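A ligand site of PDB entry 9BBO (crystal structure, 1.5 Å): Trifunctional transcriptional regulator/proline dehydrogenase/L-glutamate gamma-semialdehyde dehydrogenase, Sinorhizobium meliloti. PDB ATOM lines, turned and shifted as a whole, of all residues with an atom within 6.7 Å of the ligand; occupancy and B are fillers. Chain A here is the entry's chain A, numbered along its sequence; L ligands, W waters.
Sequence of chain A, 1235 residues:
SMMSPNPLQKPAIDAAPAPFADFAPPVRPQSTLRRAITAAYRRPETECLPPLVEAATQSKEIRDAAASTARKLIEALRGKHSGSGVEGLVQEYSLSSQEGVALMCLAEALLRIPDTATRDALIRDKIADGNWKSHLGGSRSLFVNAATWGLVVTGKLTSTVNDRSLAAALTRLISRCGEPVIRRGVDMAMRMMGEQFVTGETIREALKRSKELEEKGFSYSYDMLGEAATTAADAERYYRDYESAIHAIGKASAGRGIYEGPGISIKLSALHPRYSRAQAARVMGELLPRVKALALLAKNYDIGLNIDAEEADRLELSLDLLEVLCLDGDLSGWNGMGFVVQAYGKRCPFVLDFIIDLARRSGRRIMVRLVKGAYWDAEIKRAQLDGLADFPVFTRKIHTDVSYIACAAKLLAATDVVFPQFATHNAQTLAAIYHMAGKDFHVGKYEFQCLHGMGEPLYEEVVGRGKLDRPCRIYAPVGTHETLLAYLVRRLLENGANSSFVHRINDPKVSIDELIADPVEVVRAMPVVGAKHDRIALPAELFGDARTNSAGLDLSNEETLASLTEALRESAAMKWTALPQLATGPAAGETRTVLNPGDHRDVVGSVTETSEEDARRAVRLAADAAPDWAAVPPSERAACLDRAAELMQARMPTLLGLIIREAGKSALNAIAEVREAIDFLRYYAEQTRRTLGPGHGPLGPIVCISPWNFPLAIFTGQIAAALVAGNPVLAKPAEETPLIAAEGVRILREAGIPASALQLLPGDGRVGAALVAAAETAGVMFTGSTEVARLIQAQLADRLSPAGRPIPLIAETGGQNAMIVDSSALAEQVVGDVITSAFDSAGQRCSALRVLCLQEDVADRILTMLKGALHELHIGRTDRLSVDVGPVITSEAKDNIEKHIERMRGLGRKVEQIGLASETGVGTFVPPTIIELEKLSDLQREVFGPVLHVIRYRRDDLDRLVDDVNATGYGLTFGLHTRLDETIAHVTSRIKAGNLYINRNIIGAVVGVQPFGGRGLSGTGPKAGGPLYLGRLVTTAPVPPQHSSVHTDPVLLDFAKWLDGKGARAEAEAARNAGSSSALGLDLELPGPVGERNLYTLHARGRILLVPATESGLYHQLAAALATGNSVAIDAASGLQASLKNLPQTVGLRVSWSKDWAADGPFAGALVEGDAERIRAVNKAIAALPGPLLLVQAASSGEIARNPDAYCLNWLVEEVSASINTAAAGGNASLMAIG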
ATOM      1  N   GLU A 676      17.463  20.464 -23.124  1.00  0.00           N
ATOM      2  CA  GLU A 676      16.788  21.648 -22.607  1.00  0.00           C
ATOM      3  C   GLU A 676      17.808  22.647 -22.071  1.00  0.00           C
ATOM      4  O   GLU A 676      17.656  23.864 -22.265  1.00  0.00           O
ATOM      5  CB  GLU A 676      15.798  21.253 -21.516  1.00  0.00           C
ATOM      6  CG  GLU A 676      14.944  22.409 -21.039  1.00  0.00           C
ATOM      7  CD  GLU A 676      13.766  21.967 -20.192  1.00  0.00           C
ATOM      8  OE1 GLU A 676      13.437  20.765 -20.182  1.00  0.00           O
ATOM      9  OE2 GLU A 676      13.137  22.838 -19.540  1.00  0.00           O
ATOM     10  N   PHE A 680      18.054  26.441 -23.424  1.00  0.00           N
ATOM     11  CA  PHE A 680      18.019  27.647 -22.596  1.00  0.00           C
ATOM     12  C   PHE A 680      19.199  28.555 -22.924  1.00  0.00           C
ATOM     13  O   PHE A 680      19.041  29.771 -23.087  1.00  0.00           O
ATOM     14  CB  PHE A 680      18.063  27.289 -21.106  1.00  0.00           C
ATOM     15  CG  PHE A 680      16.733  26.950 -20.499  1.00  0.00           C
ATOM     16  CD1 PHE A 680      15.637  27.779 -20.645  1.00  0.00           C
ATOM     17  CD2 PHE A 680      16.602  25.790 -19.745  1.00  0.00           C
ATOM     18  CE1 PHE A 680      14.431  27.458 -20.054  1.00  0.00           C
ATOM     19  CE2 PHE A 680      15.411  25.466 -19.155  1.00  0.00           C
ATOM     20  CZ  PHE A 680      14.320  26.288 -19.302  1.00  0.00           C
ATOM     21  N   PRO A 707      16.033  23.165  -8.460  1.00  0.00           N
ATOM     22  CA  PRO A 707      15.437  21.956  -7.889  1.00  0.00           C
ATOM     23  C   PRO A 707      16.217  20.704  -8.228  1.00  0.00           C
ATOM     24  O   PRO A 707      17.146  20.758  -9.047  1.00  0.00           O
ATOM     25  CB  PRO A 707      14.051  21.958  -8.537  1.00  0.00           C
ATOM     26  CG  PRO A 707      14.328  22.478  -9.926  1.00  0.00           C
ATOM     27  CD  PRO A 707      15.368  23.566  -9.719  1.00  0.00           C
ATOM     28  N   ASN A 709      14.778  17.935  -9.471  1.00  0.00           N
ATOM     29  CA  ASN A 709      14.102  17.150 -10.484  1.00  0.00           C
ATOM     30  C   ASN A 709      14.536  17.512 -11.900  1.00  0.00           C
ATOM     31  O   ASN A 709      14.384  16.691 -12.809  1.00  0.00           O
ATOM     32  CB  ASN A 709      12.588  17.282 -10.320  1.00  0.00           C
ATOM     33  CG  ASN A 709      12.052  18.631 -10.725  1.00  0.00           C
ATOM     34  OD1 ASN A 709      12.752  19.641 -10.688  1.00  0.00           O
ATOM     35  ND2 ASN A 709      10.771  18.662 -11.093  1.00  0.00           N
ATOM     36  N   PHE A 710      15.078  18.708 -12.099  1.00  0.00           N
ATOM     37  CA  PHE A 710      15.756  19.091 -13.341  1.00  0.00           C
ATOM     38  C   PHE A 710      17.066  19.746 -12.952  1.00  0.00           C
ATOM     39  O   PHE A 710      17.249  20.966 -13.071  1.00  0.00           O
ATOM     40  CB  PHE A 710      14.878  19.992 -14.207  1.00  0.00           C
ATOM     41  CG  PHE A 710      13.753  19.246 -14.864  1.00  0.00           C
ATOM     42  CD1 PHE A 710      13.966  18.581 -16.049  1.00  0.00           C
ATOM     43  CD2 PHE A 710      12.505  19.170 -14.261  1.00  0.00           C
ATOM     44  CE1 PHE A 710      12.943  17.870 -16.664  1.00  0.00           C
ATOM     45  CE2 PHE A 710      11.474  18.451 -14.868  1.00  0.00           C
ATOM     46  CZ  PHE A 710      11.690  17.805 -16.068  1.00  0.00           C
ATOM     47  N   ILE A 714      16.965  23.233 -15.318  1.00  0.00           N
ATOM     48  CA  ILE A 714      16.437  24.429 -14.661  1.00  0.00           C
ATOM     49  C   ILE A 714      17.565  25.173 -13.952  1.00  0.00           C
ATOM     50  O   ILE A 714      17.580  26.413 -13.908  1.00  0.00           O
ATOM     51  CB  ILE A 714      15.292  24.054 -13.710  1.00  0.00           C
ATOM     52  CG1 ILE A 714      14.069  23.619 -14.534  1.00  0.00           C
ATOM     53  CG2 ILE A 714      14.932  25.229 -12.798  1.00  0.00           C
ATOM     54  CD1 ILE A 714      12.845  23.203 -13.721  1.00  0.00           C
ATOM     55  N   THR A 783      12.909  27.828  -8.066  1.00  0.00           N
ATOM     56  CA  THR A 783      12.000  26.791  -8.550  1.00  0.00           C
ATOM     57  C   THR A 783      11.973  25.685  -7.518  1.00  0.00           C
ATOM     58  O   THR A 783      13.024  25.138  -7.161  1.00  0.00           O
ATOM     59  CB  THR A 783      12.451  26.265  -9.923  1.00  0.00           C
ATOM     60  OG1 THR A 783      12.537  27.346 -10.858  1.00  0.00           O
ATOM     61  CG2 THR A 783      11.448  25.237 -10.447  1.00  0.00           C
ATOM     62  N   GLU A 812       8.670  29.620  -9.531  1.00  0.00           N
ATOM     63  CA  GLU A 812       7.897  28.613 -10.247  1.00  0.00           C
ATOM     64  C   GLU A 812       7.657  27.462  -9.280  1.00  0.00           C
ATOM     65  O   GLU A 812       8.607  26.899  -8.730  1.00  0.00           O
ATOM     66  CB  GLU A 812       8.644  28.132 -11.490  1.00  0.00           C
ATOM     67  N   GLY A 814       5.002  24.561  -9.289  1.00  0.00           N
ATOM     68  CA  GLY A 814       4.258  23.299  -9.434  1.00  0.00           C
ATOM     69  C   GLY A 814       2.785  23.456  -9.796  1.00  0.00           C
ATOM     70  O   GLY A 814       2.336  24.502 -10.251  1.00  0.00           O
ATOM     71  N   GLN A 844       7.962  12.962 -11.098  1.00  0.00           N
ATOM     72  CA  GLN A 844       8.669  14.069 -10.446  1.00  0.00           C
ATOM     73  C   GLN A 844       8.847  15.260 -11.358  1.00  0.00           C
ATOM     74  O   GLN A 844       9.902  15.920 -11.334  1.00  0.00           O
ATOM     75  CB  GLN A 844      10.010  13.561  -9.910  1.00  0.00           C
ATOM     76  CG  GLN A 844       9.859  12.542  -8.788  1.00  0.00           C
ATOM     77  CD  GLN A 844      11.187  11.976  -8.301  1.00  0.00           C
ATOM     78  OE1 GLN A 844      11.383  11.791  -7.103  1.00  0.00           O
ATOM     79  NE2 GLN A 844      12.104  11.706  -9.208  1.00  0.00           N
ATOM     80  N   ARG A 845       7.874  15.542 -12.204  1.00  0.00           N
ATOM     81  CA  ARG A 845       7.822  16.764 -12.971  1.00  0.00           C
ATOM     82  C   ARG A 845       6.754  17.656 -12.376  1.00  0.00           C
ATOM     83  O   ARG A 845       5.668  17.190 -12.027  1.00  0.00           O
ATOM     84  CB  ARG A 845       7.479  16.498 -14.443  1.00  0.00           C
ATOM     85  CG  ARG A 845       8.492  15.663 -15.188  1.00  0.00           C
ATOM     86  CD  ARG A 845       8.015  15.514 -16.613  1.00  0.00           C
ATOM     87  NE  ARG A 845       8.919  14.693 -17.407  1.00  0.00           N
ATOM     88  CZ  ARG A 845       9.714  15.157 -18.352  1.00  0.00           C
ATOM     89  NH1 ARG A 845       9.769  16.443 -18.660  1.00  0.00           N
ATOM     90  NH2 ARG A 845      10.487  14.293 -19.022  1.00  0.00           N
ATOM     91  N   CYS A 846       7.048  18.951 -12.273  1.00  0.00           N
ATOM     92  CA  CYS A 846       5.981  19.861 -11.861  1.00  0.00           C
ATOM     93  C   CYS A 846       4.823  19.877 -12.850  1.00  0.00           C
ATOM     94  O   CYS A 846       3.697  20.179 -12.456  1.00  0.00           O
ATOM     95  CB  CYS A 846       6.532  21.271 -11.660  1.00  0.00           C
ATOM     96  SG  CYS A 846       7.626  21.326 -10.221  1.00  0.00           S
ATOM     97  N   SER A 847       5.089  19.524 -14.108  1.00  0.00           N
ATOM     98  CA  SER A 847       4.113  19.419 -15.186  1.00  0.00           C
ATOM     99  C   SER A 847       3.333  18.113 -15.188  1.00  0.00           C
ATOM    100  O   SER A 847       2.429  17.970 -16.016  1.00  0.00           O
ATOM    101  CB  SER A 847       4.837  19.521 -16.524  1.00  0.00           C
ATOM    102  OG  SER A 847       5.864  18.518 -16.557  1.00  0.00           O
ATOM    103  N   ALA A 848       3.676  17.160 -14.328  1.00  0.00           N
ATOM    104  CA  ALA A 848       3.133  15.809 -14.458  1.00  0.00           C
ATOM    105  C   ALA A 848       1.624  15.773 -14.314  1.00  0.00           C
ATOM    106  O   ALA A 848       1.020  16.560 -13.573  1.00  0.00           O
ATOM    107  CB  ALA A 848       3.769  14.873 -13.426  1.00  0.00           C
ATOM    108  N   PHE A 944       4.080  14.419  -5.158  1.00  0.00           N
ATOM    109  CA  PHE A 944       5.134  14.583  -6.174  1.00  0.00           C
ATOM    110  C   PHE A 944       5.790  13.227  -6.461  1.00  0.00           C
ATOM    111  O   PHE A 944       6.962  12.980  -6.180  1.00  0.00           O
ATOM    112  CB  PHE A 944       6.168  15.600  -5.706  1.00  0.00           C
ATOM    113  CG  PHE A 944       6.830  16.340  -6.828  1.00  0.00           C
ATOM    114  CD1 PHE A 944       6.115  17.269  -7.570  1.00  0.00           C
ATOM    115  CD2 PHE A 944       8.174  16.136  -7.119  1.00  0.00           C
ATOM    116  CE1 PHE A 944       6.730  17.958  -8.593  1.00  0.00           C
ATOM    117  CE2 PHE A 944       8.791  16.838  -8.138  1.00  0.00           C
ATOM    118  CZ  PHE A 944       8.062  17.736  -8.890  1.00  0.00           C
ATOM    119  N   LEU A 972      -0.794  25.313 -13.916  1.00  0.00           N
ATOM    120  CA  LEU A 972       0.464  25.068 -14.607  1.00  0.00           C
ATOM    121  C   LEU A 972       0.190  24.379 -15.946  1.00  0.00           C
ATOM    122  O   LEU A 972       0.006  25.060 -16.951  1.00  0.00           O
ATOM    123  CB  LEU A 972       1.415  24.253 -13.725  1.00  0.00           C
ATOM    124  CG  LEU A 972       2.853  24.123 -14.244  1.00  0.00           C
ATOM    125  CD1 LEU A 972       3.454  25.475 -14.647  1.00  0.00           C
ATOM    126  CD2 LEU A 972       3.711  23.452 -13.183  1.00  0.00           C
ATOM    127  N   THR A 973       0.109  23.050 -15.975  1.00  0.00           N
ATOM    128  CA  THR A 973      -0.160  22.365 -17.230  1.00  0.00           C
ATOM    129  C   THR A 973      -1.576  21.805 -17.224  1.00  0.00           C
ATOM    130  O   THR A 973      -2.174  21.565 -16.179  1.00  0.00           O
ATOM    131  CB  THR A 973       0.837  21.218 -17.484  1.00  0.00           C
ATOM    132  OG1 THR A 973       0.761  20.267 -16.415  1.00  0.00           O
ATOM    133  CG2 THR A 973       2.274  21.734 -17.629  1.00  0.00           C
ATOM    134  N   ASN A 995       0.176  26.376 -19.498  1.00  0.00           N
ATOM    135  CA  ASN A 995       0.644  25.489 -20.563  1.00  0.00           C
ATOM    136  C   ASN A 995      -0.463  24.505 -20.895  1.00  0.00           C
ATOM    137  O   ASN A 995      -0.721  23.589 -20.119  1.00  0.00           O
ATOM    138  CB  ASN A 995       1.924  24.761 -20.156  1.00  0.00           C
ATOM    139  CG  ASN A 995       3.152  25.642 -20.326  1.00  0.00           C
ATOM    140  OD1 ASN A 995       3.496  26.418 -19.440  1.00  0.00           O
ATOM    141  ND2 ASN A 995       3.774  25.570 -21.497  1.00  0.00           N
ATOM    142  N   TYR A 997      -2.225  21.734 -23.603  1.00  0.00           N
ATOM    143  CA  TYR A 997      -1.819  20.701 -24.544  1.00  0.00           C
ATOM    144  C   TYR A 997      -3.054  19.988 -25.066  1.00  0.00           C
ATOM    145  O   TYR A 997      -3.870  19.527 -24.267  1.00  0.00           O
ATOM    146  CB  TYR A 997      -0.870  19.696 -23.878  1.00  0.00           C
ATOM    147  CG  TYR A 997       0.410  20.314 -23.395  1.00  0.00           C
ATOM    148  CD1 TYR A 997       1.465  20.526 -24.271  1.00  0.00           C
ATOM    149  CD2 TYR A 997       0.577  20.686 -22.058  1.00  0.00           C
ATOM    150  CE1 TYR A 997       2.683  21.086 -23.827  1.00  0.00           C
ATOM    151  CE2 TYR A 997       1.774  21.254 -21.602  1.00  0.00           C
ATOM    152  CZ  TYR A 997       2.816  21.436 -22.497  1.00  0.00           C
ATOM    153  OH  TYR A 997       3.997  21.993 -22.044  1.00  0.00           O
ATOM    154  N   ILE A1002       1.332  16.146 -21.686  1.00  0.00           N
ATOM    155  CA  ILE A1002       1.393  17.474 -21.072  1.00  0.00           C
ATOM    156  C   ILE A1002       2.771  17.765 -20.490  1.00  0.00           C
ATOM    157  O   ILE A1002       2.909  18.701 -19.703  1.00  0.00           O
ATOM    158  CB  ILE A1002       0.285  17.677 -20.018  1.00  0.00           C
ATOM    159  CG1 ILE A1002       0.467  16.797 -18.780  1.00  0.00           C
ATOM    160  CG2 ILE A1002      -1.094  17.469 -20.626  1.00  0.00           C
ATOM    161  CD1 ILE A1002      -0.488  17.150 -17.649  1.00  0.00           C
ATOM    162  N   ILE A1003       3.795  17.003 -20.868  1.00  0.00           N
ATOM    163  CA  ILE A1003       5.127  17.163 -20.295  1.00  0.00           C
ATOM    164  C   ILE A1003       6.143  17.531 -21.363  1.00  0.00           C
ATOM    165  O   ILE A1003       5.894  17.465 -22.565  1.00  0.00           O
ATOM    166  CB  ILE A1003       5.583  15.901 -19.530  1.00  0.00           C
ATOM    167  CG1 ILE A1003       5.677  14.690 -20.453  1.00  0.00           C
ATOM    168  CG2 ILE A1003       4.649  15.606 -18.387  1.00  0.00           C
ATOM    169  CD1 ILE A1003       6.503  13.535 -19.832  1.00  0.00           C
ATOM    170  N   GLY A1004       7.334  17.903 -20.904  1.00  0.00           N
ATOM    171  CA  GLY A1004       8.428  18.140 -21.813  1.00  0.00           C
ATOM    172  C   GLY A1004       8.295  19.408 -22.629  1.00  0.00           C
ATOM    173  O   GLY A1004       8.597  19.408 -23.831  1.00  0.00           O
ATOM    174  N   ALA A1005       7.854  20.499 -22.004  1.00  0.00           N
ATOM    175  CA  ALA A1005       7.781  21.780 -22.680  1.00  0.00           C
ATOM    176  C   ALA A1005       9.136  22.107 -23.311  1.00  0.00           C
ATOM    177  O   ALA A1005      10.185  21.874 -22.701  1.00  0.00           O
ATOM    178  CB  ALA A1005       7.352  22.873 -21.699  1.00  0.00           C
ATOM    179  N   VAL A1006       9.096  22.650 -24.525  1.00  0.00           N
ATOM    180  CA  VAL A1006      10.284  22.931 -25.317  1.00  0.00           C
ATOM    181  C   VAL A1006      10.576  24.434 -25.276  1.00  0.00           C
ATOM    182  O   VAL A1006       9.693  25.250 -25.540  1.00  0.00           O
ATOM    183  CB  VAL A1006      10.116  22.428 -26.766  1.00  0.00           C
ATOM    184  CG1 VAL A1006      11.252  22.893 -27.659  1.00  0.00           C
ATOM    185  CG2 VAL A1006       9.994  20.904 -26.792  1.00  0.00           C
ATOM    186  N   PHE A1012       7.421  28.018 -20.663  1.00  0.00           N
ATOM    187  CA  PHE A1012       6.887  27.206 -19.584  1.00  0.00           C
ATOM    188  C   PHE A1012       6.675  28.011 -18.314  1.00  0.00           C
ATOM    189  O   PHE A1012       7.599  28.692 -17.834  1.00  0.00           O
ATOM    190  CB  PHE A1012       7.810  26.033 -19.261  1.00  0.00           C
ATOM    191  CG  PHE A1012       7.234  25.120 -18.243  1.00  0.00           C
ATOM    192  CD1 PHE A1012       6.223  24.237 -18.597  1.00  0.00           C
ATOM    193  CD2 PHE A1012       7.688  25.133 -16.922  1.00  0.00           C
ATOM    194  CE1 PHE A1012       5.668  23.388 -17.654  1.00  0.00           C
ATOM    195  CE2 PHE A1012       7.131  24.270 -15.983  1.00  0.00           C
ATOM    196  CZ  PHE A1012       6.120  23.393 -16.356  1.00  0.00           C
HETATM  197  N1  LIG L   1       9.432  21.956 -17.952  1.00  0.00           N
HETATM  198  C1  LIG L   1       9.171  20.624 -17.438  1.00  0.00           C
HETATM  199  C2  LIG L   1       8.149  19.946 -18.283  1.00  0.00           C
HETATM  200  O1  LIG L   1       7.989  18.695 -18.174  1.00  0.00           O
HETATM  201  C3  LIG L   1       8.723  20.668 -16.014  1.00  0.00           C
HETATM  202  C4  LIG L   1       9.697  21.483 -15.189  1.00  0.00           C
HETATM  203  C5  LIG L   1       9.482  21.250 -13.724  1.00  0.00           C
HETATM  204  O2  LIG L   1       9.205  20.097 -13.291  1.00  0.00           O
HETATM  205  O3  LIG L   1       9.574  22.206 -12.899  1.00  0.00           O
HETATM  206  O4  LIG L   1       7.440  20.610 -19.096  1.00  0.00           O
HETATM  207  O   HOH W   1       4.714  20.865 -19.815  1.00  0.00           O
HETATM  208  O   HOH W   2      11.168  21.894 -10.577  1.00  0.00           O
HETATM  209  O   HOH W   3      10.623  20.678 -20.316  1.00  0.00           O
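N of Cys 846 lies within hydrogen-bond range of O2 of the ligand, 2.6 Å away.
The side-chain sulfur of Cys 846 lies close to an oxygen (O3) of the ligand, at 3.4 Å.
OG of Ser 847 sits at hydrogen-bond distance from O1 of the ligand.
O1 of the ligand lies within salt-bridge range of NH1 of Arg 845 (2.9 Å).
O1 of the ligand is in hydrogen-bond range of N of Gly 1004, at 2.9 Å.
The backbone NH of Ala 1005 sits at hydrogen-bond distance from an oxygen (O4) of the ligand, at 2.9 Å.
The side-chain amide nitrogen (ND2) of Asn 709 is in hydrogen-bond range of an oxygen (O2) of the ligand (3.1 Å).
The backbone carbonyl oxygen (O) of Ser 847 is in hydrogen-bond range of the side-chain hydroxyl (OG1) of Thr 973 (2.9 Å).
The side-chain amide nitrogen (ND2) of Asn 709 sits at hydrogen-bond distance from the backbone carbonyl oxygen (O) of Gln 844 (2.9 Å).
CE2 of Phe 710 touches O2 of the ligand, at 3.2 Å.
Ile 714 touches the ligand.
Ile 1003 touches the ligand (C to O1, 3.9 Å).
Phe 1012 touches the ligand (CE1 to O4, 3.6 Å).
Hydrophobic or aromatic side chains that line the ligand: Phe 710, Ile 714, Ile 1003, Ala 1005 and Phe 1012.
Ten residues have an atom within 4 Å of the ligand: Asn 709, Phe 710, Ile 714, Arg 845, Cys 846, Ser 847, Ile 1003, Gly 1004, Ala 1005 and Phe 1012.
The nearest printed residue that does not touch the ligand is Glu 676 (4.1 Å).
Water W1 lies within hydrogen-bond range of the side-chain hydroxyl of Tyr 997 (2.6 Å), the backbone carbonyl oxygen of Ile 1002 (2.8 Å) and an oxygen (O4) of the ligand (2.8 Å).
Water W2 lies within hydrogen-bond range of OD1 of Asn 709, O3 of the ligand and SG of Cys 846.
Water W3 lies within hydrogen-bond range of the backbone carbonyl oxygen (O) of Ala 1005 (2.7 Å), the side-chain carboxylate (OE1) of Glu 676 (2.8 Å) and a nitrogen (N1) of the ligand (2.9 Å).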
